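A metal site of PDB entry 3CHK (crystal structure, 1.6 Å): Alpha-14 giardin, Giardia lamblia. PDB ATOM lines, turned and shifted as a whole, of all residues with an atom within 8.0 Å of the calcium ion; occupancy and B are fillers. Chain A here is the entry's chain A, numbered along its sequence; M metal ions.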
ATOM      1  N   LEU A 171     -11.688 -12.790  -1.981  1.00  0.00           N
ATOM      2  CA  LEU A 171     -11.389 -13.842  -2.951  1.00  0.00           C
ATOM      3  C   LEU A 171     -11.957 -15.203  -2.524  1.00  0.00           C
ATOM      4  O   LEU A 171     -12.502 -15.949  -3.347  1.00  0.00           O
ATOM      5  CB  LEU A 171      -9.882 -13.919  -3.142  1.00  0.00           C
ATOM      6  CG  LEU A 171      -9.308 -12.703  -3.889  1.00  0.00           C
ATOM      7  CD1 LEU A 171      -7.800 -12.771  -3.848  1.00  0.00           C
ATOM      8  CD2 LEU A 171      -9.797 -12.712  -5.364  1.00  0.00           C
ATOM      9  N   VAL A 172     -11.853 -15.536  -1.242  1.00  0.00           N
ATOM     10  CA  VAL A 172     -12.424 -16.821  -0.808  1.00  0.00           C
ATOM     11  C   VAL A 172     -13.954 -16.801  -0.813  1.00  0.00           C
ATOM     12  O   VAL A 172     -14.608 -17.794  -1.112  1.00  0.00           O
ATOM     13  CB  VAL A 172     -11.807 -17.321   0.543  1.00  0.00           C
ATOM     14  CG1 VAL A 172     -12.437 -16.658   1.777  1.00  0.00           C
ATOM     15  CG2 VAL A 172     -11.865 -18.862   0.627  1.00  0.00           C
ATOM     16  N   ARG A 173     -14.544 -15.665  -0.457  1.00  0.00           N
ATOM     17  CA  ARG A 173     -15.984 -15.544  -0.552  1.00  0.00           C
ATOM     18  C   ARG A 173     -16.437 -15.778  -1.993  1.00  0.00           C
ATOM     19  O   ARG A 173     -17.417 -16.501  -2.205  1.00  0.00           O
ATOM     20  CB  ARG A 173     -16.474 -14.178  -0.087  1.00  0.00           C
ATOM     21  CG  ARG A 173     -17.986 -14.009  -0.241  1.00  0.00           C
ATOM     22  CD  ARG A 173     -18.733 -14.924   0.718  1.00  0.00           C
ATOM     23  NE  ARG A 173     -20.183 -14.661   0.666  1.00  0.00           N
ATOM     24  CZ  ARG A 173     -21.057 -15.217   1.501  1.00  0.00           C
ATOM     25  NH1 ARG A 173     -20.624 -16.046   2.443  1.00  0.00           N
ATOM     26  NH2 ARG A 173     -22.355 -14.928   1.416  1.00  0.00           N
ATOM     27  N   LYS A 174     -15.750 -15.153  -2.959  1.00  0.00           N
ATOM     28  CA  LYS A 174     -16.024 -15.311  -4.383  1.00  0.00           C
ATOM     29  C   LYS A 174     -15.957 -16.778  -4.800  1.00  0.00           C
ATOM     30  O   LYS A 174     -16.891 -17.330  -5.397  1.00  0.00           O
ATOM     31  CB  LYS A 174     -15.064 -14.485  -5.242  1.00  0.00           C
ATOM     32  CG  LYS A 174     -15.377 -14.529  -6.770  1.00  0.00           C
ATOM     33  CD  LYS A 174     -14.597 -15.641  -7.516  1.00  0.00           C
ATOM     34  CE  LYS A 174     -14.739 -15.539  -9.044  1.00  0.00           C
ATOM     35  NZ  LYS A 174     -14.132 -16.726  -9.731  1.00  0.00           N
ATOM     36  N   ALA A 175     -14.843 -17.412  -4.424  1.00  0.00           N
ATOM     37  CA  ALA A 175     -14.674 -18.846  -4.605  1.00  0.00           C
ATOM     38  C   ALA A 175     -15.845 -19.664  -4.043  1.00  0.00           C
ATOM     39  O   ALA A 175     -16.301 -20.607  -4.688  1.00  0.00           O
ATOM     40  CB  ALA A 175     -13.352 -19.317  -3.995  1.00  0.00           C
ATOM     41  N   ILE A 176     -16.324 -19.320  -2.858  1.00  0.00           N
ATOM     42  CA  ILE A 176     -17.368 -20.062  -2.170  1.00  0.00           C
ATOM     43  C   ILE A 176     -18.695 -19.844  -2.951  1.00  0.00           C
ATOM     44  O   ILE A 176     -19.513 -20.752  -3.077  1.00  0.00           O
ATOM     45  CB  ILE A 176     -17.451 -19.620  -0.682  1.00  0.00           C
ATOM     46  CG1 ILE A 176     -16.288 -20.271   0.104  1.00  0.00           C
ATOM     47  CG2 ILE A 176     -18.744 -20.047  -0.032  1.00  0.00           C
ATOM     48  CD1 ILE A 176     -15.969 -19.632   1.436  1.00  0.00           C
ATOM     49  N   GLU A 177     -18.857 -18.646  -3.487  1.00  0.00           N
ATOM     50  CA  GLU A 177     -20.105 -18.319  -4.160  1.00  0.00           C
ATOM     51  C   GLU A 177     -20.287 -19.002  -5.507  1.00  0.00           C
ATOM     52  O   GLU A 177     -21.429 -19.211  -5.938  1.00  0.00           O
ATOM     53  CB  GLU A 177     -20.316 -16.818  -4.251  1.00  0.00           C
ATOM     54  CG  GLU A 177     -20.707 -16.178  -2.912  1.00  0.00           C
ATOM     55  CD  GLU A 177     -20.662 -14.655  -2.978  1.00  0.00           C
ATOM     56  OE1 GLU A 177     -20.880 -13.991  -1.951  1.00  0.00           O
ATOM     57  OE2 GLU A 177     -20.384 -14.119  -4.073  1.00  0.00           O
ATOM     58  N   THR A 178     -19.204 -19.378  -6.171  1.00  0.00           N
ATOM     59  CA  THR A 178     -19.310 -20.007  -7.504  1.00  0.00           C
ATOM     60  C   THR A 178     -19.356 -21.525  -7.364  1.00  0.00           C
ATOM     61  O   THR A 178     -18.632 -22.104  -6.555  1.00  0.00           O
ATOM     62  CB  THR A 178     -18.118 -19.653  -8.409  1.00  0.00           C
ATOM     63  OG1 THR A 178     -16.915 -20.171  -7.817  1.00  0.00           O
ATOM     64  CG2 THR A 178     -17.973 -18.151  -8.587  1.00  0.00           C
ATOM     65  N   LYS A 179     -20.203 -22.193  -8.148  1.00  0.00           N
ATOM     66  CA  LYS A 179     -20.275 -23.649  -8.084  1.00  0.00           C
ATOM     67  C   LYS A 179     -19.047 -24.245  -8.783  1.00  0.00           C
ATOM     68  O   LYS A 179     -18.663 -23.808  -9.878  1.00  0.00           O
ATOM     69  CB  LYS A 179     -21.560 -24.157  -8.742  1.00  0.00           C
ATOM     70  CG  LYS A 179     -21.882 -25.602  -8.394  1.00  0.00           C
ATOM     71  CD  LYS A 179     -23.275 -26.006  -8.883  1.00  0.00           C
ATOM     72  CE  LYS A 179     -23.913 -27.010  -7.924  1.00  0.00           C
ATOM     73  NZ  LYS A 179     -24.151 -26.368  -6.585  1.00  0.00           N
ATOM     74  N   GLY A 180     -18.418 -25.217  -8.105  1.00  0.00           N
ATOM     75  CA  GLY A 180     -17.163 -25.803  -8.583  1.00  0.00           C
ATOM     76  C   GLY A 180     -15.941 -24.936  -8.314  1.00  0.00           C
ATOM     77  O   GLY A 180     -16.044 -23.714  -8.132  1.00  0.00           O
ATOM     78  N   VAL A 181     -14.779 -25.566  -8.282  1.00  0.00           N
ATOM     79  CA  VAL A 181     -13.542 -24.806  -8.215  1.00  0.00           C
ATOM     80  C   VAL A 181     -13.253 -24.287  -9.612  1.00  0.00           C
ATOM     81  O   VAL A 181     -13.021 -25.078 -10.522  1.00  0.00           O
ATOM     82  CB  VAL A 181     -12.377 -25.709  -7.745  1.00  0.00           C
ATOM     83  CG1 VAL A 181     -11.083 -24.918  -7.669  1.00  0.00           C
ATOM     84  CG2 VAL A 181     -12.703 -26.358  -6.407  1.00  0.00           C
ATOM     85  N   LYS A 182     -13.272 -22.957  -9.776  1.00  0.00           N
ATOM     86  CA  LYS A 182     -12.894 -22.315 -11.042  1.00  0.00           C
ATOM     87  C   LYS A 182     -11.384 -22.163 -11.147  1.00  0.00           C
ATOM     88  O   LYS A 182     -10.688 -22.152 -10.131  1.00  0.00           O
ATOM     89  CB  LYS A 182     -13.551 -20.929 -11.166  1.00  0.00           C
ATOM     90  CG  LYS A 182     -15.051 -20.907 -11.001  1.00  0.00           C
ATOM     91  CD  LYS A 182     -15.784 -21.907 -11.878  1.00  0.00           C
ATOM     92  CE  LYS A 182     -17.273 -21.599 -11.892  1.00  0.00           C
ATOM     93  NZ  LYS A 182     -18.041 -22.616 -12.664  1.00  0.00           N
ATOM     94  N   LYS A 183     -10.891 -22.007 -12.382  1.00  0.00           N
ATOM     95  CA  LYS A 183      -9.464 -21.837 -12.645  1.00  0.00           C
ATOM     96  C   LYS A 183      -8.770 -20.799 -11.773  1.00  0.00           C
ATOM     97  O   LYS A 183      -7.705 -21.057 -11.241  1.00  0.00           O
ATOM     98  CB  LYS A 183      -9.200 -21.518 -14.126  1.00  0.00           C
ATOM     99  CG  LYS A 183      -7.826 -21.927 -14.582  1.00  0.00           C
ATOM    100  CD  LYS A 183      -7.303 -21.043 -15.723  1.00  0.00           C
ATOM    101  CE  LYS A 183      -5.817 -21.320 -16.008  1.00  0.00           C
ATOM    102  NZ  LYS A 183      -4.951 -21.194 -14.779  1.00  0.00           N
ATOM    103  N   ASP A 184      -9.383 -19.622 -11.617  1.00  0.00           N
ATOM    104  CA  ASP A 184      -8.794 -18.494 -10.882  1.00  0.00           C
ATOM    105  C   ASP A 184      -8.947 -18.645  -9.370  1.00  0.00           C
ATOM    106  O   ASP A 184      -8.338 -17.898  -8.598  1.00  0.00           O
ATOM    107  CB  ASP A 184      -9.473 -17.196 -11.338  1.00  0.00           C
ATOM    108  CG  ASP A 184     -10.961 -17.160 -11.032  1.00  0.00           C
ATOM    109  OD1 ASP A 184     -11.724 -17.959 -11.611  1.00  0.00           O
ATOM    110  OD2 ASP A 184     -11.395 -16.320 -10.205  1.00  0.00           O
ATOM    111  N   GLU A 185      -9.737 -19.627  -8.974  1.00  0.00           N
ATOM    112  CA  GLU A 185     -10.017 -19.933  -7.562  1.00  0.00           C
ATOM    113  C   GLU A 185      -9.022 -20.918  -6.979  1.00  0.00           C
ATOM    114  O   GLU A 185      -8.872 -20.961  -5.747  1.00  0.00           O
ATOM    115  CB  GLU A 185     -11.436 -20.433  -7.409  1.00  0.00           C
ATOM    116  CG  GLU A 185     -12.435 -19.325  -7.671  1.00  0.00           C
ATOM    117  CD  GLU A 185     -13.856 -19.797  -7.795  1.00  0.00           C
ATOM    118  OE1 GLU A 185     -14.156 -20.946  -7.454  1.00  0.00           O
ATOM    119  OE2 GLU A 185     -14.708 -18.995  -8.236  1.00  0.00           O
ATOM    120  N   VAL A 186      -8.359 -21.687  -7.835  1.00  0.00           N
ATOM    121  CA  VAL A 186      -7.390 -22.674  -7.345  1.00  0.00           C
ATOM    122  C   VAL A 186      -6.357 -22.063  -6.440  1.00  0.00           C
ATOM    123  O   VAL A 186      -6.119 -22.576  -5.337  1.00  0.00           O
ATOM    124  CB  VAL A 186      -6.685 -23.486  -8.492  1.00  0.00           C
ATOM    125  CG1 VAL A 186      -5.698 -24.504  -7.867  1.00  0.00           C
ATOM    126  CG2 VAL A 186      -7.723 -24.247  -9.285  1.00  0.00           C
ATOM    127  N   TRP A 189      -7.717 -21.081  -2.815  1.00  0.00           N
ATOM    128  CA  TRP A 189      -7.876 -22.196  -1.875  1.00  0.00           C
ATOM    129  C   TRP A 189      -6.500 -22.696  -1.414  1.00  0.00           C
ATOM    130  O   TRP A 189      -6.289 -22.988  -0.246  1.00  0.00           O
ATOM    131  CB  TRP A 189      -8.599 -23.327  -2.562  1.00  0.00           C
ATOM    132  CG  TRP A 189     -10.067 -23.068  -2.726  1.00  0.00           C
ATOM    133  CD1 TRP A 189     -10.756 -22.968  -3.904  1.00  0.00           C
ATOM    134  CD2 TRP A 189     -11.023 -22.924  -1.688  1.00  0.00           C
ATOM    135  NE1 TRP A 189     -12.098 -22.813  -3.659  1.00  0.00           N
ATOM    136  CE2 TRP A 189     -12.297 -22.765  -2.310  1.00  0.00           C
ATOM    137  CE3 TRP A 189     -10.955 -22.950  -0.275  1.00  0.00           C
ATOM    138  CZ2 TRP A 189     -13.461 -22.581  -1.569  1.00  0.00           C
ATOM    139  CZ3 TRP A 189     -12.105 -22.780   0.440  1.00  0.00           C
ATOM    140  CH2 TRP A 189     -13.350 -22.609  -0.214  1.00  0.00           C
ATOM    141  N   GLY A 220     -18.224 -23.096   3.621  1.00  0.00           N
ATOM    142  CA  GLY A 220     -17.780 -22.779   2.277  1.00  0.00           C
ATOM    143  C   GLY A 220     -17.023 -23.952   1.705  1.00  0.00           C
ATOM    144  O   GLY A 220     -17.249 -24.343   0.552  1.00  0.00           O
ATOM    145  N   ASP A 223     -19.519 -26.694   0.793  1.00  0.00           N
ATOM    146  CA  ASP A 223     -20.166 -26.288  -0.470  1.00  0.00           C
ATOM    147  C   ASP A 223     -19.283 -26.568  -1.696  1.00  0.00           C
ATOM    148  O   ASP A 223     -19.770 -27.091  -2.711  1.00  0.00           O
ATOM    149  CB  ASP A 223     -20.469 -24.767  -0.477  1.00  0.00           C
ATOM    150  CG  ASP A 223     -21.578 -24.343   0.473  1.00  0.00           C
ATOM    151  OD1 ASP A 223     -22.264 -25.212   1.038  1.00  0.00           O
ATOM    152  OD2 ASP A 223     -21.756 -23.077   0.628  1.00  0.00           O
ATOM    153  N   GLU A 224     -17.996 -26.211  -1.603  1.00  0.00           N
ATOM    154  CA  GLU A 224     -17.111 -26.141  -2.750  1.00  0.00           C
ATOM    155  C   GLU A 224     -16.617 -27.523  -3.181  1.00  0.00           C
ATOM    156  O   GLU A 224     -16.548 -27.814  -4.384  1.00  0.00           O
ATOM    157  CB  GLU A 224     -15.927 -25.185  -2.456  1.00  0.00           C
ATOM    158  CG  GLU A 224     -14.920 -24.970  -3.599  1.00  0.00           C
ATOM    159  CD  GLU A 224     -15.388 -23.971  -4.678  1.00  0.00           C
ATOM    160  OE1 GLU A 224     -16.604 -23.956  -4.976  1.00  0.00           O
ATOM    161  OE2 GLU A 224     -14.565 -23.248  -5.231  1.00  0.00           O
ATOM    162  N   PHE A 225     -16.295 -28.364  -2.203  1.00  0.00           N
ATOM    163  CA  PHE A 225     -15.563 -29.601  -2.473  1.00  0.00           C
ATOM    164  C   PHE A 225     -16.410 -30.818  -2.213  1.00  0.00           C
ATOM    165  O   PHE A 225     -17.394 -30.762  -1.488  1.00  0.00           O
ATOM    166  CB  PHE A 225     -14.303 -29.650  -1.585  1.00  0.00           C
ATOM    167  CG  PHE A 225     -13.326 -28.530  -1.848  1.00  0.00           C
ATOM    168  CD1 PHE A 225     -12.511 -28.554  -2.951  1.00  0.00           C
ATOM    169  CD2 PHE A 225     -13.222 -27.443  -0.951  1.00  0.00           C
ATOM    170  CE1 PHE A 225     -11.609 -27.523  -3.215  1.00  0.00           C
ATOM    171  CE2 PHE A 225     -12.340 -26.404  -1.211  1.00  0.00           C
ATOM    172  CZ  PHE A 225     -11.519 -26.429  -2.334  1.00  0.00           C
HETATM  173 CA    CA M   1     -16.131 -21.984  -6.557  1.00  0.00          CA
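Within 4 Å of the calcium ion: Ala 175, Thr 178, Gly 180, Glu 185 and Glu 224.
Along chain A the residues within 4 Å of the calcium ion span positions 175 to 224.
The nearest printed residue that does not touch the calcium ion is Val 181 (4.2 Å).
OE1 of Glu 185 lies close to N of Lys 182 (3.2 Å).
OE2 of Glu 185 is in salt-bridge range of NZ of Lys 174, 2.8 Å away.
NE1 of Trp 189 sits close to OE2 of Glu 224 (3.0 Å).
The calcium ion is bound by the backbone carbonyl oxygen (O) of Ala 175, the backbone carbonyl oxygen (O) of Gly 180, the side-chain hydroxyl (OG1) of Thr 178, the side-chain carboxylate (OE1) of Glu 185, the side-chain carboxylate (OE2) of Glu 224, the backbone carbonyl oxygen (O) of Thr 178 and the side-chain carboxylate (OE1) of Glu 224.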
